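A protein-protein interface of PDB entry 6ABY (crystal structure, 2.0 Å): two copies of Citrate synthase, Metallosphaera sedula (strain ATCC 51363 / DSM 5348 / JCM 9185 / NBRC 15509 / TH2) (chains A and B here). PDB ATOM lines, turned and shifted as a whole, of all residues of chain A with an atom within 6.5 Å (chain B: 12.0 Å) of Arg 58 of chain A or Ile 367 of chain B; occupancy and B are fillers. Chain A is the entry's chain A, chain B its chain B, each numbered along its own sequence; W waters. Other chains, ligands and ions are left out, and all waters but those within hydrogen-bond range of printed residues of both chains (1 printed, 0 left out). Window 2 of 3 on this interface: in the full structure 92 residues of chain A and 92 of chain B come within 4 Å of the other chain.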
ATOM      1  N   GLU A  45      13.057 -19.321 -17.139  1.00  0.00           N
ATOM      2  CA  GLU A  45      13.358 -18.718 -15.826  1.00  0.00           C
ATOM      3  C   GLU A  45      13.178 -17.194 -15.902  1.00  0.00           C
ATOM      4  O   GLU A  45      12.667 -16.631 -14.922  1.00  0.00           O
ATOM      5  CB  GLU A  45      14.748 -19.094 -15.336  1.00  0.00           C
ATOM      6  CG  GLU A  45      15.040 -18.552 -13.962  1.00  0.00           C
ATOM      7  CD  GLU A  45      16.385 -19.012 -13.419  1.00  0.00           C
ATOM      8  OE1 GLU A  45      17.416 -18.374 -13.777  1.00  0.00           O
ATOM      9  OE2 GLU A  45      16.394 -20.014 -12.654  1.00  0.00           O
ATOM     10  N   PRO A  56      12.129 -18.386  -9.732  1.00  0.00           N
ATOM     11  CA  PRO A  56      11.336 -19.522  -9.296  1.00  0.00           C
ATOM     12  C   PRO A  56      12.188 -20.575  -8.574  1.00  0.00           C
ATOM     13  O   PRO A  56      13.342 -20.753  -8.923  1.00  0.00           O
ATOM     14  CB  PRO A  56      10.826 -20.134 -10.602  1.00  0.00           C
ATOM     15  CG  PRO A  56      11.910 -19.787 -11.596  1.00  0.00           C
ATOM     16  CD  PRO A  56      12.447 -18.444 -11.166  1.00  0.00           C
ATOM     17  N   THR A  57      11.566 -21.283  -7.635  1.00  0.00           N
ATOM     18  CA  THR A  57      12.124 -22.531  -7.058  1.00  0.00           C
ATOM     19  C   THR A  57      12.180 -23.578  -8.171  1.00  0.00           C
ATOM     20  O   THR A  57      11.489 -23.392  -9.232  1.00  0.00           O
ATOM     21  CB  THR A  57      11.269 -23.033  -5.892  1.00  0.00           C
ATOM     22  OG1 THR A  57      10.042 -23.432  -6.504  1.00  0.00           O
ATOM     23  CG2 THR A  57      11.074 -21.988  -4.814  1.00  0.00           C
ATOM     24  N   ARG A  58      12.927 -24.661  -7.926  1.00  0.00           N
ATOM     25  CA  ARG A  58      12.956 -25.856  -8.798  1.00  0.00           C
ATOM     26  C   ARG A  58      11.509 -26.235  -9.153  1.00  0.00           C
ATOM     27  O   ARG A  58      11.224 -26.392 -10.328  1.00  0.00           O
ATOM     28  CB  ARG A  58      13.713 -27.007  -8.122  1.00  0.00           C
ATOM     29  CG  ARG A  58      13.915 -28.252  -8.975  1.00  0.00           C
ATOM     30  CD  ARG A  58      14.933 -28.062 -10.096  1.00  0.00           C
ATOM     31  NE  ARG A  58      14.293 -27.608 -11.327  1.00  0.00           N
ATOM     32  CZ  ARG A  58      14.923 -27.110 -12.401  1.00  0.00           C
ATOM     33  NH1 ARG A  58      16.238 -27.007 -12.413  1.00  0.00           N
ATOM     34  NH2 ARG A  58      14.231 -26.704 -13.458  1.00  0.00           N
ATOM     35  N   HIS A  59      10.634 -26.401  -8.155  1.00  0.00           N
ATOM     36  CA  HIS A  59       9.226 -26.856  -8.341  1.00  0.00           C
ATOM     37  C   HIS A  59       8.493 -25.842  -9.232  1.00  0.00           C
ATOM     38  O   HIS A  59       7.871 -26.269 -10.215  1.00  0.00           O
ATOM     39  CB  HIS A  59       8.517 -27.073  -6.990  1.00  0.00           C
ATOM     40  CG  HIS A  59       7.047 -27.335  -7.100  1.00  0.00           C
ATOM     41  ND1 HIS A  59       6.532 -28.424  -7.783  1.00  0.00           N
ATOM     42  CD2 HIS A  59       5.980 -26.662  -6.610  1.00  0.00           C
ATOM     43  CE1 HIS A  59       5.218 -28.412  -7.721  1.00  0.00           C
ATOM     44  NE2 HIS A  59       4.853 -27.336  -7.004  1.00  0.00           N
ATOM     45  N   GLU A  60       8.583 -24.553  -8.901  1.00  0.00           N
ATOM     46  CA  GLU A  60       7.843 -23.485  -9.637  1.00  0.00           C
ATOM     47  C   GLU A  60       8.311 -23.490 -11.099  1.00  0.00           C
ATOM     48  O   GLU A  60       7.447 -23.490 -11.962  1.00  0.00           O
ATOM     49  CB  GLU A  60       8.013 -22.115  -9.010  1.00  0.00           C
ATOM     50  CG  GLU A  60       7.308 -21.974  -7.677  1.00  0.00           C
ATOM     51  CD  GLU A  60       7.750 -20.761  -6.869  1.00  0.00           C
ATOM     52  OE1 GLU A  60       8.858 -20.241  -7.113  1.00  0.00           O
ATOM     53  OE2 GLU A  60       6.980 -20.322  -6.016  1.00  0.00           O
ATOM     54  N   LEU A  61       9.607 -23.678 -11.354  1.00  0.00           N
ATOM     55  CA  LEU A  61      10.132 -23.567 -12.737  1.00  0.00           C
ATOM     56  C   LEU A  61       9.703 -24.800 -13.527  1.00  0.00           C
ATOM     57  O   LEU A  61       9.374 -24.644 -14.688  1.00  0.00           O
ATOM     58  CB  LEU A  61      11.656 -23.429 -12.733  1.00  0.00           C
ATOM     59  CG  LEU A  61      12.269 -23.249 -14.114  1.00  0.00           C
ATOM     60  CD1 LEU A  61      11.645 -22.041 -14.808  1.00  0.00           C
ATOM     61  CD2 LEU A  61      13.788 -23.083 -14.023  1.00  0.00           C
ATOM     62  N   ASP A  62       9.708 -25.987 -12.908  1.00  0.00           N
ATOM     63  CA  ASP A  62       9.294 -27.234 -13.603  1.00  0.00           C
ATOM     64  C   ASP A  62       7.833 -27.091 -14.036  1.00  0.00           C
ATOM     65  O   ASP A  62       7.559 -27.349 -15.232  1.00  0.00           O
ATOM     66  CB  ASP A  62       9.568 -28.478 -12.752  1.00  0.00           C
ATOM     67  CG  ASP A  62      11.056 -28.825 -12.678  1.00  0.00           C
ATOM     68  OD1 ASP A  62      11.790 -28.460 -13.617  1.00  0.00           O
ATOM     69  OD2 ASP A  62      11.472 -29.441 -11.672  1.00  0.00           O
ATOM     70  N   ASP A  63       6.956 -26.656 -13.122  1.00  0.00           N
ATOM     71  CA  ASP A  63       5.505 -26.435 -13.384  1.00  0.00           C
ATOM     72  C   ASP A  63       5.351 -25.366 -14.488  1.00  0.00           C
ATOM     73  O   ASP A  63       4.568 -25.577 -15.450  1.00  0.00           O
ATOM     74  CB  ASP A  63       4.746 -26.040 -12.103  1.00  0.00           C
ATOM     75  CG  ASP A  63       4.504 -27.179 -11.098  1.00  0.00           C
ATOM     76  OD1 ASP A  63       4.766 -28.374 -11.443  1.00  0.00           O
ATOM     77  OD2 ASP A  63       4.019 -26.880  -9.973  1.00  0.00           O
ATOM     78  N   LYS A  65       7.530 -24.380 -16.832  1.00  0.00           N
ATOM     79  CA  LYS A  65       8.048 -24.866 -18.137  1.00  0.00           C
ATOM     80  C   LYS A  65       6.999 -25.786 -18.772  1.00  0.00           C
ATOM     81  O   LYS A  65       6.902 -25.795 -20.021  1.00  0.00           O
ATOM     82  CB  LYS A  65       9.367 -25.629 -18.003  1.00  0.00           C
ATOM     83  CG  LYS A  65      10.611 -24.769 -17.856  1.00  0.00           C
ATOM     84  CD  LYS A  65      11.747 -25.488 -17.162  1.00  0.00           C
ATOM     85  CE  LYS A  65      12.036 -26.856 -17.737  1.00  0.00           C
ATOM     86  NZ  LYS A  65      12.245 -27.860 -16.659  1.00  0.00           N
ATOM     87  N   ARG B 363      22.426 -10.220  -6.530  1.00  0.00           N
ATOM     88  CA  ARG B 363      23.191 -11.465  -6.838  1.00  0.00           C
ATOM     89  C   ARG B 363      22.235 -12.497  -7.439  1.00  0.00           C
ATOM     90  O   ARG B 363      21.127 -12.654  -6.911  1.00  0.00           O
ATOM     91  CB  ARG B 363      23.845 -12.014  -5.562  1.00  0.00           C
ATOM     92  CG  ARG B 363      24.804 -13.158  -5.832  1.00  0.00           C
ATOM     93  CD  ARG B 363      25.382 -13.706  -4.551  1.00  0.00           C
ATOM     94  NE  ARG B 363      24.436 -14.574  -3.885  1.00  0.00           N
ATOM     95  CZ  ARG B 363      24.386 -15.902  -4.024  1.00  0.00           C
ATOM     96  NH1 ARG B 363      25.210 -16.528  -4.848  1.00  0.00           N
ATOM     97  NH2 ARG B 363      23.502 -16.599  -3.331  1.00  0.00           N
ATOM     98  N   TYR B 364      22.616 -13.117  -8.555  1.00  0.00           N
ATOM     99  CA  TYR B 364      21.883 -14.272  -9.113  1.00  0.00           C
ATOM    100  C   TYR B 364      22.015 -15.444  -8.113  1.00  0.00           C
ATOM    101  O   TYR B 364      23.119 -15.908  -7.834  1.00  0.00           O
ATOM    102  CB  TYR B 364      22.374 -14.603 -10.519  1.00  0.00           C
ATOM    103  CG  TYR B 364      21.652 -15.770 -11.109  1.00  0.00           C
ATOM    104  CD1 TYR B 364      22.100 -17.068 -10.885  1.00  0.00           C
ATOM    105  CD2 TYR B 364      20.464 -15.593 -11.806  1.00  0.00           C
ATOM    106  CE1 TYR B 364      21.406 -18.156 -11.389  1.00  0.00           C
ATOM    107  CE2 TYR B 364      19.790 -16.669 -12.363  1.00  0.00           C
ATOM    108  CZ  TYR B 364      20.259 -17.957 -12.135  1.00  0.00           C
ATOM    109  OH  TYR B 364      19.574 -19.025 -12.605  1.00  0.00           O
ATOM    110  N   VAL B 365      20.899 -15.849  -7.517  1.00  0.00           N
ATOM    111  CA  VAL B 365      20.810 -16.952  -6.517  1.00  0.00           C
ATOM    112  C   VAL B 365      20.530 -18.203  -7.325  1.00  0.00           C
ATOM    113  O   VAL B 365      19.525 -18.278  -8.036  1.00  0.00           O
ATOM    114  CB  VAL B 365      19.728 -16.713  -5.440  1.00  0.00           C
ATOM    115  CG1 VAL B 365      19.611 -17.885  -4.445  1.00  0.00           C
ATOM    116  CG2 VAL B 365      19.980 -15.405  -4.691  1.00  0.00           C
ATOM    117  N   PRO B 366      21.443 -19.197  -7.289  1.00  0.00           N
ATOM    118  CA  PRO B 366      21.224 -20.440  -8.018  1.00  0.00           C
ATOM    119  C   PRO B 366      19.943 -21.118  -7.504  1.00  0.00           C
ATOM    120  O   PRO B 366      19.653 -21.004  -6.339  1.00  0.00           O
ATOM    121  CB  PRO B 366      22.497 -21.281  -7.758  1.00  0.00           C
ATOM    122  CG  PRO B 366      23.231 -20.595  -6.615  1.00  0.00           C
ATOM    123  CD  PRO B 366      22.681 -19.189  -6.497  1.00  0.00           C
ATOM    124  N   ILE B 367      19.245 -21.838  -8.375  1.00  0.00           N
ATOM    125  CA  ILE B 367      17.891 -22.388  -8.118  1.00  0.00           C
ATOM    126  C   ILE B 367      17.891 -23.328  -6.893  1.00  0.00           C
ATOM    127  O   ILE B 367      16.939 -23.235  -6.115  1.00  0.00           O
ATOM    128  CB  ILE B 367      17.331 -23.044  -9.390  1.00  0.00           C
ATOM    129  CG1 ILE B 367      15.820 -23.269  -9.240  1.00  0.00           C
ATOM    130  CG2 ILE B 367      18.096 -24.300  -9.771  1.00  0.00           C
ATOM    131  CD1 ILE B 367      15.101 -23.571 -10.533  1.00  0.00           C
ATOM    132  N   GLU B 368      18.931 -24.138  -6.657  1.00  0.00           N
ATOM    133  CA  GLU B 368      18.971 -25.079  -5.489  1.00  0.00           C
ATOM    134  C   GLU B 368      19.038 -24.283  -4.157  1.00  0.00           C
ATOM    135  O   GLU B 368      18.735 -24.846  -3.097  1.00  0.00           O
ATOM    136  CB  GLU B 368      20.115 -26.077  -5.664  1.00  0.00           C
ATOM    137  CG  GLU B 368      21.495 -25.437  -5.439  1.00  0.00           C
ATOM    138  CD  GLU B 368      22.189 -24.792  -6.656  1.00  0.00           C
ATOM    139  OE1 GLU B 368      21.511 -24.594  -7.727  1.00  0.00           O
ATOM    140  OE2 GLU B 368      23.429 -24.481  -6.533  1.00  0.00           O
ATOM    141  N   GLU B 369      19.387 -22.994  -4.180  1.00  0.00           N
ATOM    142  CA  GLU B 369      19.385 -22.140  -2.960  1.00  0.00           C
ATOM    143  C   GLU B 369      18.062 -21.395  -2.727  1.00  0.00           C
ATOM    144  O   GLU B 369      17.937 -20.831  -1.659  1.00  0.00           O
ATOM    145  CB  GLU B 369      20.499 -21.102  -3.006  1.00  0.00           C
ATOM    146  CG  GLU B 369      21.894 -21.707  -2.959  1.00  0.00           C
ATOM    147  CD  GLU B 369      23.009 -20.664  -2.929  1.00  0.00           C
ATOM    148  OE1 GLU B 369      22.686 -19.452  -2.788  1.00  0.00           O
ATOM    149  OE2 GLU B 369      24.184 -21.048  -3.125  1.00  0.00           O
ATOM    150  N   ARG B 370      17.074 -21.446  -3.609  1.00  0.00           N
ATOM    151  CA  ARG B 370      15.878 -20.556  -3.519  1.00  0.00           C
ATOM    152  C   ARG B 370      14.839 -21.148  -2.541  1.00  0.00           C
ATOM    153  O   ARG B 370      14.569 -22.355  -2.640  1.00  0.00           O
ATOM    154  CB  ARG B 370      15.287 -20.373  -4.925  1.00  0.00           C
ATOM    155  CG  ARG B 370      16.149 -19.505  -5.824  1.00  0.00           C
ATOM    156  CD  ARG B 370      15.683 -19.467  -7.267  1.00  0.00           C
ATOM    157  NE  ARG B 370      16.787 -19.100  -8.151  1.00  0.00           N
ATOM    158  CZ  ARG B 370      16.796 -19.333  -9.451  1.00  0.00           C
ATOM    159  NH1 ARG B 370      17.877 -19.062 -10.177  1.00  0.00           N
ATOM    160  NH2 ARG B 370      15.718 -19.850 -10.023  1.00  0.00           N
ATOM    161  N   LEU B 371      14.216 -20.316  -1.691  1.00  0.00           N
ATOM    162  CA  LEU B 371      13.322 -20.738  -0.559  1.00  0.00           C
ATOM    163  C   LEU B 371      13.615 -22.197  -0.177  1.00  0.00           C
ATOM    164  O   LEU B 371      14.449 -22.467   0.682  1.00  0.00           O
ATOM    165  CB  LEU B 371      11.844 -20.574  -0.936  1.00  0.00           C
ATOM    166  CG  LEU B 371      10.838 -21.141   0.078  1.00  0.00           C
ATOM    167  CD1 LEU B 371      10.772 -20.280   1.340  1.00  0.00           C
ATOM    168  CD2 LEU B 371       9.449 -21.288  -0.536  1.00  0.00           C
HETATM  169  O   HOH W   1      14.594 -24.460  -5.611  1.00  0.00           O
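O of Pro 56 of chain A lies within hydrogen-bond range of NH2 of Arg 370 of chain B. The guanidinium group of Arg 370 of chain B is in salt-bridge range of the side-chain carboxylate of Glu 45 of chain A. The side-chain hydroxyl of Tyr 364 of chain B lies within hydrogen-bond range of the side-chain carboxylate of Glu 45 of chain A, 2.5 Å away.
The backbone carbonyl oxygen (O) of Val 365 of chain B sits at hydrogen-bond distance from the guanidinium group (NH1) of Arg 370 of chain B (2.8 Å). The side-chain carboxylate (OD1) of Asp 62 of chain A is in salt-bridge range of the guanidinium group (NH2) of Arg 58 of chain A, 3.0 Å away. OH of Tyr 364 of chain B lies within hydrogen-bond range of NH1 of Arg 370 of chain B. The backbone NH of Thr 57 of chain A is in hydrogen-bond range of the side-chain carboxylate of Glu 60 of chain A (2.9 Å). N of His 59 of chain A lies close to OG1 of Thr 57 of chain A (3.4 Å).
O of Pro 56 of chain A touches CG1 of Ile 367 of chain B, 3.5 Å away. CD1 of Ile 367 of chain B touches C of Thr 57 of chain A (3.8 Å). Arg 58 of chain A touches Ile 367 of chain B. Ile 367 of chain B touches Leu 61 of chain A.
Ile 367 of chain B touches four residues of chain A. Pro 56 of chain A touches just these residues of chain B: Ile 367 (3.5 Å) and Arg 370 (2.8 Å). No residue of chain B comes within 4 Å of Glu 60 of chain A. Of the printed residues of chain B, Leu 61 of chain A touches Ile 367. Asp 62 of chain A touches none of the printed residues of chain B. Printed residues of chain A within 4 Å of Tyr 364 of chain B: Glu 45. Of the printed residues of chain A, Arg 370 of chain B touches Glu 45 (2.7 Å) and Pro 56 (2.8 Å). Printed residues of chain B within 4 Å of Glu 45 of chain A: Tyr 364 (2.5 Å) and Arg 370 (2.7 Å). Lys 65 of chain A touches none of the printed residues of chain B. Glu 369 of chain B touches none of the printed residues of chain A. The nearest residue of chain B that does not touch Arg 58 of chain A is Arg 370 of chain B (5.7 Å). The nearest printed residue of chain B that does not touch Glu 45 of chain A is Ile 367 of chain B (4.3 Å).
Printed residues of chain B that touch a printed residue of chain A: Tyr 364, Ile 367 and Arg 370. Hydrophobic or aromatic side chains of chain A within 4 Å of the printed part of chain B: Pro 56 and Leu 61. Among the printed residues, Asp or Glu carboxylates within 4 Å of a Lys or Arg side-chain nitrogen of the other chain: Glu 45 of chain A with Arg 370 of chain B.
No position is printed for both chains.
Water W1 bridges the backbone carbonyl oxygen of Ile 367 of chain B and the backbone NH of Arg 58 of chain A.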
